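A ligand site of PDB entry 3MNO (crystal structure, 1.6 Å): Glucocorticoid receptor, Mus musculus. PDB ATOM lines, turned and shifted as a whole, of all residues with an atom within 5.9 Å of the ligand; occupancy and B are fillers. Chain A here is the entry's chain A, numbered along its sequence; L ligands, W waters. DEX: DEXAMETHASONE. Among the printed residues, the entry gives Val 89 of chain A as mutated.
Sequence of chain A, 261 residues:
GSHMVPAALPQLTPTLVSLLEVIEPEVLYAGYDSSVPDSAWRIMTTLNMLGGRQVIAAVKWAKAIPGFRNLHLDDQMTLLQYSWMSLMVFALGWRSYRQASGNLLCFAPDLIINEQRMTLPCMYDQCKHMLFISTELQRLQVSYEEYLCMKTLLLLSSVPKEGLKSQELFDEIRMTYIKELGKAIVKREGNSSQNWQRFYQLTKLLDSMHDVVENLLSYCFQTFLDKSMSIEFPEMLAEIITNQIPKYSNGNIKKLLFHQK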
ATOM      1  N   MET A  44      14.201  33.581  28.760  1.00  0.00           N
ATOM      2  CA  MET A  44      13.710  32.222  28.466  1.00  0.00           C
ATOM      3  C   MET A  44      13.743  31.871  26.968  1.00  0.00           C
ATOM      4  O   MET A  44      14.148  30.766  26.583  1.00  0.00           O
ATOM      5  CB  MET A  44      12.289  32.061  29.033  1.00  0.00           C
ATOM      6  CG  MET A  44      12.328  31.892  30.535  1.00  0.00           C
ATOM      7  SD  MET A  44      10.632  31.623  31.229  1.00  0.00           S
ATOM      8  CE  MET A  44      10.191  33.225  31.600  1.00  0.00           C
ATOM      9  N   THR A  45      13.293  32.799  26.113  1.00  0.00           N
ATOM     10  CA  THR A  45      13.344  32.528  24.686  1.00  0.00           C
ATOM     11  C   THR A  45      14.791  32.277  24.221  1.00  0.00           C
ATOM     12  O   THR A  45      15.052  31.344  23.470  1.00  0.00           O
ATOM     13  CB  THR A  45      12.705  33.710  23.930  1.00  0.00           C
ATOM     14  OG1 THR A  45      11.291  33.641  24.141  1.00  0.00           O
ATOM     15  CG2 THR A  45      13.017  33.613  22.416  1.00  0.00           C
ATOM     16  N   LEU A  47      17.279  31.238  25.984  1.00  0.00           N
ATOM     17  CA  LEU A  47      17.767  29.941  26.482  1.00  0.00           C
ATOM     18  C   LEU A  47      17.245  28.811  25.594  1.00  0.00           C
ATOM     19  O   LEU A  47      17.954  27.840  25.335  1.00  0.00           O
ATOM     20  CB  LEU A  47      17.332  29.672  27.932  1.00  0.00           C
ATOM     21  CG  LEU A  47      17.837  30.692  28.948  1.00  0.00           C
ATOM     22  CD1 LEU A  47      17.379  30.220  30.308  1.00  0.00           C
ATOM     23  CD2 LEU A  47      19.373  30.886  28.929  1.00  0.00           C
ATOM     24  N   ASN A  48      15.976  28.877  25.219  1.00  0.00           N
ATOM     25  CA  ASN A  48      15.406  27.856  24.371  1.00  0.00           C
ATOM     26  C   ASN A  48      16.129  27.784  23.031  1.00  0.00           C
ATOM     27  O   ASN A  48      16.308  26.680  22.477  1.00  0.00           O
ATOM     28  CB  ASN A  48      13.897  28.097  24.160  1.00  0.00           C
ATOM     29  CG  ASN A  48      13.086  27.796  25.407  1.00  0.00           C
ATOM     30  OD1 ASN A  48      13.392  26.855  26.148  1.00  0.00           O
ATOM     31  ND2 ASN A  48      11.974  28.509  25.568  1.00  0.00           N
ATOM     32  N   LEU A  50      19.219  28.536  22.365  1.00  0.00           N
ATOM     33  CA  LEU A  50      20.494  27.854  22.625  1.00  0.00           C
ATOM     34  C   LEU A  50      20.234  26.376  22.864  1.00  0.00           C
ATOM     35  O   LEU A  50      20.957  25.486  22.368  1.00  0.00           O
ATOM     36  CB  LEU A  50      21.164  28.466  23.839  1.00  0.00           C
ATOM     37  CG  LEU A  50      22.374  27.750  24.431  1.00  0.00           C
ATOM     38  CD1 LEU A  50      23.507  27.712  23.352  1.00  0.00           C
ATOM     39  CD2 LEU A  50      22.853  28.403  25.700  1.00  0.00           C
ATOM     40  N   GLY A  51      19.206  26.068  23.659  1.00  0.00           N
ATOM     41  CA  GLY A  51      18.895  24.677  23.973  1.00  0.00           C
ATOM     42  C   GLY A  51      18.628  23.827  22.730  1.00  0.00           C
ATOM     43  O   GLY A  51      18.994  22.645  22.713  1.00  0.00           O
ATOM     44  N   GLY A  52      17.976  24.397  21.703  1.00  0.00           N
ATOM     45  CA  GLY A  52      17.709  23.592  20.519  1.00  0.00           C
ATOM     46  C   GLY A  52      19.031  23.193  19.862  1.00  0.00           C
ATOM     47  O   GLY A  52      19.171  22.050  19.406  1.00  0.00           O
ATOM     48  N   GLN A  54      21.936  22.893  21.416  1.00  0.00           N
ATOM     49  CA  GLN A  54      22.566  21.896  22.279  1.00  0.00           C
ATOM     50  C   GLN A  54      21.932  20.508  22.107  1.00  0.00           C
ATOM     51  O   GLN A  54      22.640  19.462  22.148  1.00  0.00           O
ATOM     52  CB  GLN A  54      22.482  22.340  23.746  1.00  0.00           C
ATOM     53  CG  GLN A  54      23.315  23.523  24.124  1.00  0.00           C
ATOM     54  CD  GLN A  54      22.993  24.000  25.524  1.00  0.00           C
ATOM     55  OE1 GLN A  54      22.156  23.413  26.208  1.00  0.00           O
ATOM     56  NE2 GLN A  54      23.689  25.022  25.972  1.00  0.00           N
ATOM     57  N   VAL A  55      20.608  20.428  21.933  1.00  0.00           N
ATOM     58  CA  VAL A  55      19.953  19.162  21.742  1.00  0.00           C
ATOM     59  C   VAL A  55      20.367  18.509  20.413  1.00  0.00           C
ATOM     60  O   VAL A  55      20.614  17.311  20.368  1.00  0.00           O
ATOM     61  CB  VAL A  55      18.428  19.240  21.923  1.00  0.00           C
ATOM     62  CG1 VAL A  55      17.759  17.943  21.511  1.00  0.00           C
ATOM     63  CG2 VAL A  55      18.124  19.585  23.383  1.00  0.00           C
ATOM     64  N   TRP A  84      16.414  14.219  27.152  1.00  0.00           N
ATOM     65  CA  TRP A  84      17.044  15.466  26.753  1.00  0.00           C
ATOM     66  C   TRP A  84      17.202  16.507  27.864  1.00  0.00           C
ATOM     67  O   TRP A  84      18.256  17.139  28.015  1.00  0.00           O
ATOM     68  CB  TRP A  84      16.418  16.077  25.493  1.00  0.00           C
ATOM     69  CG  TRP A  84      15.114  16.760  25.710  1.00  0.00           C
ATOM     70  CD1 TRP A  84      13.887  16.161  25.762  1.00  0.00           C
ATOM     71  CD2 TRP A  84      14.898  18.150  26.020  1.00  0.00           C
ATOM     72  NE1 TRP A  84      12.911  17.101  26.004  1.00  0.00           N
ATOM     73  CE2 TRP A  84      13.521  18.320  26.243  1.00  0.00           C
ATOM     74  CE3 TRP A  84      15.768  19.224  26.246  1.00  0.00           C
ATOM     75  CZ2 TRP A  84      12.968  19.560  26.580  1.00  0.00           C
ATOM     76  CZ3 TRP A  84      15.237  20.464  26.555  1.00  0.00           C
ATOM     77  CH2 TRP A  84      13.817  20.616  26.717  1.00  0.00           C
ATOM     78  N   MET A  85      16.149  16.687  28.669  1.00  0.00           N
ATOM     79  CA  MET A  85      16.243  17.717  29.699  1.00  0.00           C
ATOM     80  C   MET A  85      17.297  17.379  30.722  1.00  0.00           C
ATOM     81  O   MET A  85      18.133  18.239  31.096  1.00  0.00           O
ATOM     82  CB  MET A  85      14.877  17.958  30.354  1.00  0.00           C
ATOM     83  CG  MET A  85      14.930  19.044  31.459  1.00  0.00           C
ATOM     84  SD  MET A  85      15.195  20.707  30.843  1.00  0.00           S
ATOM     85  CE  MET A  85      13.508  21.139  30.141  1.00  0.00           C
ATOM     86  N   MET A  88      20.663  18.118  29.221  1.00  0.00           N
ATOM     87  CA  MET A  88      20.970  19.547  29.141  1.00  0.00           C
ATOM     88  C   MET A  88      21.251  20.189  30.492  1.00  0.00           C
ATOM     89  O   MET A  88      22.160  21.006  30.661  1.00  0.00           O
ATOM     90  CB  MET A  88      19.833  20.325  28.442  1.00  0.00           C
ATOM     91  CG  MET A  88      19.489  19.817  27.031  1.00  0.00           C
ATOM     92  SD  MET A  88      20.917  20.114  25.950  1.00  0.00           S
ATOM     93  CE  MET A  88      21.416  18.578  25.657  1.00  0.00           C
ATOM     94  N   VAL A  89      20.462  19.806  31.488  1.00  0.00           N
ATOM     95  CA  VAL A  89      20.632  20.349  32.826  1.00  0.00           C
ATOM     96  C   VAL A  89      21.933  19.853  33.469  1.00  0.00           C
ATOM     97  O   VAL A  89      22.621  20.609  34.174  1.00  0.00           O
ATOM     98  CB  VAL A  89      19.419  19.961  33.687  1.00  0.00           C
ATOM     99  CG1 VAL A  89      19.657  20.342  35.131  1.00  0.00           C
ATOM    100  CG2 VAL A  89      18.181  20.646  33.140  1.00  0.00           C
ATOM    101  N   LEU A  92      24.733  21.806  31.875  1.00  0.00           N
ATOM    102  CA  LEU A  92      24.675  23.164  32.410  1.00  0.00           C
ATOM    103  C   LEU A  92      25.239  23.163  33.836  1.00  0.00           C
ATOM    104  O   LEU A  92      25.956  24.068  34.255  1.00  0.00           O
ATOM    105  CB  LEU A  92      23.206  23.634  32.431  1.00  0.00           C
ATOM    106  CG  LEU A  92      22.903  24.883  33.245  1.00  0.00           C
ATOM    107  CD1 LEU A  92      23.581  26.117  32.599  1.00  0.00           C
ATOM    108  CD2 LEU A  92      21.411  25.060  33.278  1.00  0.00           C
ATOM    109  N   ARG A  95      29.140  22.991  33.547  1.00  0.00           N
ATOM    110  CA  ARG A  95      29.751  24.279  33.157  1.00  0.00           C
ATOM    111  C   ARG A  95      29.668  25.256  34.318  1.00  0.00           C
ATOM    112  O   ARG A  95      30.625  25.985  34.597  1.00  0.00           O
ATOM    113  CB  ARG A  95      29.048  24.888  31.953  1.00  0.00           C
ATOM    114  CG  ARG A  95      29.148  24.000  30.732  1.00  0.00           C
ATOM    115  CD  ARG A  95      28.617  24.725  29.482  1.00  0.00           C
ATOM    116  NE  ARG A  95      27.201  25.104  29.568  1.00  0.00           N
ATOM    117  CZ  ARG A  95      26.191  24.321  29.204  1.00  0.00           C
ATOM    118  NH1 ARG A  95      26.377  23.036  28.840  1.00  0.00           N
ATOM    119  NH2 ARG A  95      24.953  24.830  29.213  1.00  0.00           N
ATOM    120  N   CYS A 106      25.969  29.099  34.015  1.00  0.00           N
ATOM    121  CA  CYS A 106      26.844  29.249  32.847  1.00  0.00           C
ATOM    122  C   CYS A 106      26.266  28.532  31.647  1.00  0.00           C
ATOM    123  O   CYS A 106      26.681  27.429  31.315  1.00  0.00           O
ATOM    124  CB  CYS A 106      28.278  28.778  33.178  1.00  0.00           C
ATOM    125  SG  CYS A 106      29.023  29.728  34.564  1.00  0.00           S
ATOM    126  N   PHE A 107      25.326  29.178  30.981  1.00  0.00           N
ATOM    127  CA  PHE A 107      24.697  28.563  29.837  1.00  0.00           C
ATOM    128  C   PHE A 107      25.666  28.399  28.704  1.00  0.00           C
ATOM    129  O   PHE A 107      25.595  27.411  27.979  1.00  0.00           O
ATOM    130  CB  PHE A 107      23.415  29.328  29.402  1.00  0.00           C
ATOM    131  CG  PHE A 107      22.263  29.126  30.350  1.00  0.00           C
ATOM    132  CD1 PHE A 107      22.058  29.988  31.406  1.00  0.00           C
ATOM    133  CD2 PHE A 107      21.406  28.021  30.215  1.00  0.00           C
ATOM    134  CE1 PHE A 107      21.012  29.797  32.321  1.00  0.00           C
ATOM    135  CE2 PHE A 107      20.360  27.830  31.130  1.00  0.00           C
ATOM    136  CZ  PHE A 107      20.216  28.688  32.194  1.00  0.00           C
ATOM    137  N   GLN A 126      12.780  28.959  38.761  1.00  0.00           N
ATOM    138  CA  GLN A 126      13.412  28.081  37.780  1.00  0.00           C
ATOM    139  C   GLN A 126      14.941  28.086  37.912  1.00  0.00           C
ATOM    140  O   GLN A 126      15.602  27.051  37.789  1.00  0.00           O
ATOM    141  CB  GLN A 126      12.984  28.450  36.344  1.00  0.00           C
ATOM    142  CG  GLN A 126      13.284  29.894  35.904  1.00  0.00           C
ATOM    143  CD  GLN A 126      12.737  30.141  34.502  1.00  0.00           C
ATOM    144  OE1 GLN A 126      13.149  29.489  33.551  1.00  0.00           O
ATOM    145  NE2 GLN A 126      11.831  31.108  34.358  1.00  0.00           N
ATOM    146  N   MET A 130      17.567  25.086  38.314  1.00  0.00           N
ATOM    147  CA  MET A 130      18.593  24.853  37.302  1.00  0.00           C
ATOM    148  C   MET A 130      19.986  24.865  37.868  1.00  0.00           C
ATOM    149  O   MET A 130      20.859  24.228  37.288  1.00  0.00           O
ATOM    150  CB  MET A 130      18.543  25.867  36.170  1.00  0.00           C
ATOM    151  CG  MET A 130      17.318  25.692  35.272  1.00  0.00           C
ATOM    152  SD  MET A 130      17.323  26.755  33.769  1.00  0.00           S
ATOM    153  CE  MET A 130      16.708  28.311  34.474  1.00  0.00           C
ATOM    154  N   ASN A 215      10.857  19.453  38.031  1.00  0.00           N
ATOM    155  CA  ASN A 215      10.589  20.872  38.261  1.00  0.00           C
ATOM    156  C   ASN A 215      10.789  21.668  36.962  1.00  0.00           C
ATOM    157  O   ASN A 215      10.001  22.542  36.579  1.00  0.00           O
ATOM    158  CB  ASN A 215      11.554  21.423  39.334  1.00  0.00           C
ATOM    159  CG  ASN A 215      11.416  20.702  40.671  1.00  0.00           C
ATOM    160  OD1 ASN A 215      10.322  20.602  41.234  1.00  0.00           O
ATOM    161  ND2 ASN A 215      12.533  20.255  41.227  1.00  0.00           N
ATOM    162  N   LEU A 216      11.833  21.303  36.226  1.00  0.00           N
ATOM    163  CA  LEU A 216      12.163  22.021  34.998  1.00  0.00           C
ATOM    164  C   LEU A 216      11.271  21.681  33.815  1.00  0.00           C
ATOM    165  O   LEU A 216      10.950  22.547  33.012  1.00  0.00           O
ATOM    166  CB  LEU A 216      13.658  21.828  34.664  1.00  0.00           C
ATOM    167  CG  LEU A 216      14.547  22.329  35.815  1.00  0.00           C
ATOM    168  CD1 LEU A 216      16.007  22.020  35.397  1.00  0.00           C
ATOM    169  CD2 LEU A 216      14.376  23.809  36.161  1.00  0.00           C
ATOM    170  N   LEU A 217      10.886  20.397  33.696  1.00  0.00           N
ATOM    171  CA  LEU A 217       9.934  20.019  32.639  1.00  0.00           C
ATOM    172  C   LEU A 217       8.583  20.718  32.861  1.00  0.00           C
ATOM    173  O   LEU A 217       7.916  21.074  31.896  1.00  0.00           O
ATOM    174  CB  LEU A 217       9.686  18.500  32.689  1.00  0.00           C
ATOM    175  CG  LEU A 217      10.862  17.709  32.113  1.00  0.00           C
ATOM    176  CD1 LEU A 217      10.573  16.198  32.262  1.00  0.00           C
ATOM    177  CD2 LEU A 217      11.101  18.078  30.667  1.00  0.00           C
ATOM    178  N   TYR A 219       8.135  23.753  33.945  1.00  0.00           N
ATOM    179  CA  TYR A 219       8.262  25.070  33.271  1.00  0.00           C
ATOM    180  C   TYR A 219       8.305  24.936  31.756  1.00  0.00           C
ATOM    181  O   TYR A 219       7.675  25.692  31.022  1.00  0.00           O
ATOM    182  CB  TYR A 219       9.539  25.796  33.727  1.00  0.00           C
ATOM    183  CG  TYR A 219       9.340  26.505  35.016  1.00  0.00           C
ATOM    184  CD1 TYR A 219       8.725  27.757  35.021  1.00  0.00           C
ATOM    185  CD2 TYR A 219       9.704  25.926  36.206  1.00  0.00           C
ATOM    186  CE1 TYR A 219       8.507  28.435  36.216  1.00  0.00           C
ATOM    187  CE2 TYR A 219       9.457  26.576  37.422  1.00  0.00           C
ATOM    188  CZ  TYR A 219       8.841  27.827  37.393  1.00  0.00           C
ATOM    189  OH  TYR A 219       8.601  28.475  38.597  1.00  0.00           O
ATOM    190  N   CYS A 220       9.097  23.990  31.280  1.00  0.00           N
ATOM    191  CA  CYS A 220       9.270  23.828  29.847  1.00  0.00           C
ATOM    192  C   CYS A 220       7.940  23.564  29.146  1.00  0.00           C
ATOM    193  O   CYS A 220       7.611  24.218  28.150  1.00  0.00           O
ATOM    194  CB  CYS A 220      10.265  22.666  29.604  1.00  0.00           C
ATOM    195  SG  CYS A 220      10.469  22.280  27.870  1.00  0.00           S
ATOM    196  N   PHE A 221       7.145  22.646  29.728  1.00  0.00           N
ATOM    197  CA  PHE A 221       5.883  22.276  29.094  1.00  0.00           C
ATOM    198  C   PHE A 221       4.866  23.404  29.176  1.00  0.00           C
ATOM    199  O   PHE A 221       4.137  23.662  28.208  1.00  0.00           O
ATOM    200  CB  PHE A 221       5.317  21.043  29.767  1.00  0.00           C
ATOM    201  CG  PHE A 221       6.149  19.784  29.580  1.00  0.00           C
ATOM    202  CD1 PHE A 221       7.124  19.704  28.576  1.00  0.00           C
ATOM    203  CD2 PHE A 221       5.849  18.658  30.323  1.00  0.00           C
ATOM    204  CE1 PHE A 221       7.879  18.495  28.398  1.00  0.00           C
ATOM    205  CE2 PHE A 221       6.598  17.451  30.157  1.00  0.00           C
ATOM    206  CZ  PHE A 221       7.589  17.401  29.214  1.00  0.00           C
ATOM    207  N   THR A 223       5.449  26.745  29.581  1.00  0.00           N
ATOM    208  CA  THR A 223       5.857  27.862  28.687  1.00  0.00           C
ATOM    209  C   THR A 223       5.734  27.495  27.205  1.00  0.00           C
ATOM    210  O   THR A 223       5.486  28.336  26.372  1.00  0.00           O
ATOM    211  CB  THR A 223       7.288  28.381  29.019  1.00  0.00           C
ATOM    212  OG1 THR A 223       8.253  27.316  28.828  1.00  0.00           O
ATOM    213  CG2 THR A 223       7.357  28.897  30.501  1.00  0.00           C
ATOM    214  N   PHE A 224       5.875  26.227  26.879  1.00  0.00           N
ATOM    215  CA  PHE A 224       5.704  25.819  25.498  1.00  0.00           C
ATOM    216  C   PHE A 224       4.207  25.834  25.130  1.00  0.00           C
ATOM    217  O   PHE A 224       3.831  26.314  24.061  1.00  0.00           O
ATOM    218  CB  PHE A 224       6.212  24.393  25.275  1.00  0.00           C
ATOM    219  CG  PHE A 224       5.949  23.890  23.874  1.00  0.00           C
ATOM    220  CD1 PHE A 224       6.648  24.419  22.787  1.00  0.00           C
ATOM    221  CD2 PHE A 224       4.937  22.962  23.650  1.00  0.00           C
ATOM    222  CE1 PHE A 224       6.366  24.015  21.491  1.00  0.00           C
ATOM    223  CE2 PHE A 224       4.660  22.537  22.352  1.00  0.00           C
ATOM    224  CZ  PHE A 224       5.342  23.078  21.286  1.00  0.00           C
ATOM    225  N   ILE A 231       6.758  32.951  24.688  1.00  0.00           N
ATOM    226  CA  ILE A 231       8.105  32.409  24.838  1.00  0.00           C
ATOM    227  C   ILE A 231       8.284  31.521  23.618  1.00  0.00           C
ATOM    228  O   ILE A 231       7.421  30.678  23.324  1.00  0.00           O
ATOM    229  CB  ILE A 231       8.242  31.610  26.138  1.00  0.00           C
ATOM    230  CG1 ILE A 231       8.113  32.588  27.324  1.00  0.00           C
ATOM    231  CG2 ILE A 231       9.604  30.832  26.159  1.00  0.00           C
ATOM    232  CD1 ILE A 231       7.961  31.919  28.663  1.00  0.00           C
ATOM    233  N   PHE A 233      10.349  28.807  20.977  1.00  0.00           N
ATOM    234  CA  PHE A 233      11.148  27.591  21.009  1.00  0.00           C
ATOM    235  C   PHE A 233      11.571  27.295  19.573  1.00  0.00           C
ATOM    236  O   PHE A 233      10.803  27.536  18.634  1.00  0.00           O
ATOM    237  CB  PHE A 233      10.309  26.409  21.490  1.00  0.00           C
ATOM    238  CG  PHE A 233       9.976  26.449  22.968  1.00  0.00           C
ATOM    239  CD1 PHE A 233       8.993  27.305  23.460  1.00  0.00           C
ATOM    240  CD2 PHE A 233      10.649  25.621  23.863  1.00  0.00           C
ATOM    241  CE1 PHE A 233       8.683  27.336  24.823  1.00  0.00           C
ATOM    242  CE2 PHE A 233      10.341  25.623  25.239  1.00  0.00           C
ATOM    243  CZ  PHE A 233       9.363  26.490  25.724  1.00  0.00           C
ATOM    244  N   LEU A 237      13.363  21.656  19.423  1.00  0.00           N
ATOM    245  CA  LEU A 237      12.774  21.549  20.745  1.00  0.00           C
ATOM    246  C   LEU A 237      11.250  21.436  20.687  1.00  0.00           C
ATOM    247  O   LEU A 237      10.662  20.629  21.387  1.00  0.00           O
ATOM    248  CB  LEU A 237      13.143  22.758  21.591  1.00  0.00           C
ATOM    249  CG  LEU A 237      13.940  22.502  22.861  1.00  0.00           C
ATOM    250  CD1 LEU A 237      14.974  21.400  22.704  1.00  0.00           C
ATOM    251  CD2 LEU A 237      14.505  23.766  23.432  1.00  0.00           C
HETATM  252  C1  DEX L   1      18.851  25.445  27.342  1.00  0.00           C
HETATM  253  C2  DEX L   1      20.213  25.620  27.323  1.00  0.00           C
HETATM  254  C3  DEX L   1      21.041  24.910  28.324  1.00  0.00           C
HETATM  255  C4  DEX L   1      20.397  24.074  29.386  1.00  0.00           C
HETATM  256  C5  DEX L   1      19.022  23.924  29.363  1.00  0.00           C
HETATM  257  C6  DEX L   1      18.370  23.135  30.438  1.00  0.00           C
HETATM  258  C7  DEX L   1      17.258  23.954  31.109  1.00  0.00           C
HETATM  259  C8  DEX L   1      16.241  24.500  30.077  1.00  0.00           C
HETATM  260  C9  DEX L   1      17.056  25.346  29.056  1.00  0.00           C
HETATM  261  C10 DEX L   1      18.133  24.492  28.332  1.00  0.00           C
HETATM  262  C11 DEX L   1      16.191  26.168  28.125  1.00  0.00           C
HETATM  263  C12 DEX L   1      15.031  26.929  28.882  1.00  0.00           C
HETATM  264  C13 DEX L   1      14.215  25.972  29.821  1.00  0.00           C
HETATM  265  C14 DEX L   1      15.175  25.325  30.836  1.00  0.00           C
HETATM  266  C15 DEX L   1      14.301  24.692  31.941  1.00  0.00           C
HETATM  267  C16 DEX L   1      13.046  25.609  31.951  1.00  0.00           C
HETATM  268  C17 DEX L   1      13.297  26.690  30.865  1.00  0.00           C
HETATM  269  C18 DEX L   1      13.357  24.900  29.053  1.00  0.00           C
HETATM  270  C19 DEX L   1      17.624  23.284  27.501  1.00  0.00           C
HETATM  271  C20 DEX L   1      11.968  27.140  30.286  1.00  0.00           C
HETATM  272  C21 DEX L   1      11.895  28.413  29.447  1.00  0.00           C
HETATM  273  C22 DEX L   1      12.965  26.227  33.355  1.00  0.00           C
HETATM  274  F1  DEX L   1      17.700  26.320  29.781  1.00  0.00           F
HETATM  275  O1  DEX L   1      22.231  25.032  28.365  1.00  0.00           O
HETATM  276  O2  DEX L   1      15.576  25.344  27.113  1.00  0.00           O
HETATM  277  O3  DEX L   1      13.911  27.902  31.300  1.00  0.00           O
HETATM  278  O4  DEX L   1      10.955  26.436  30.297  1.00  0.00           O
HETATM  279  O5  DEX L   1      10.819  28.516  28.533  1.00  0.00           O
HETATM  280  O   HOH W   1      23.549  22.088  28.374  1.00  0.00           O
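An oxygen (O1) of the ligand lies close to the side-chain amide oxygen of Gln 54, 2.7 Å away.
O2 of the ligand lies within hydrogen-bond range of OD1 of Asn 48, at 2.8 Å.
The side-chain hydroxyl of Thr 223 lies within hydrogen-bond range of an oxygen (O5) of the ligand.
An oxygen (O3) of the ligand lies within hydrogen-bond range of the side-chain amide oxygen (OE1) of Gln 126.
O1 of the ligand sits at hydrogen-bond distance from NH2 of Arg 95 (2.9 Å).
N of Cys 220 lies close to O4 of the ligand (3.2 Å).
The guanidinium group of Arg 95 lies close to the side-chain amide nitrogen of Gln 54 (3.5 Å).
SD of Met 88 sits close to OE1 of Gln 54 (3.5 Å).
The side-chain amide nitrogen (ND2) of Asn 48 lies within hydrogen-bond range of the backbone carbonyl oxygen (O) of Met 44, 3.3 Å away.
The side-chain hydroxyl of Thr 223 is in hydrogen-bond range of the backbone carbonyl oxygen of Cys 220 (3.2 Å).
The side-chain hydroxyl of Thr 223 sits at hydrogen-bond distance from the backbone carbonyl oxygen of Tyr 219 (2.8 Å).
The side-chain sulfur of Met 44 is in hydrogen-bond range of the side-chain amide nitrogen of Gln 126 (3.4 Å).
The guanidinium group of Arg 95 is in hydrogen-bond range of the backbone carbonyl oxygen of Phe 107 (2.9 Å).
The guanidinium group (NE) of Arg 95 sits at hydrogen-bond distance from the backbone carbonyl oxygen (O) of Cys 106 (3.0 Å).
The backbone carbonyl oxygen (O) of Tyr 219 sits close to an oxygen (O4) of the ligand, 3.4 Å away.
Met 44 touches the ligand.
Leu 47 touches the ligand.
Gly 51 touches the ligand.
Trp 84 touches the ligand.
SD of Met 85 touches C7 of the ligand, 3.9 Å away.
Met 88 touches the ligand (CB to C6, 3.7 Å).
Val 89 touches the ligand.
Phe 107 touches the ligand (CE2 to F1, 3.3 Å).
Met 130 touches the ligand (SD to C7, 3.9 Å).
O of Leu 216 touches C16 of the ligand, 3.9 Å away.
Ile 231 touches the ligand.
Phe 233 touches the ligand.
Hydrophobic or aromatic side chains within 4 Å of the ligand: Met 44, Leu 47, Trp 84, Met 85, Met 88, Val 89, Phe 107, Met 130, Leu 216, Tyr 219, Ile 231 and Phe 233.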
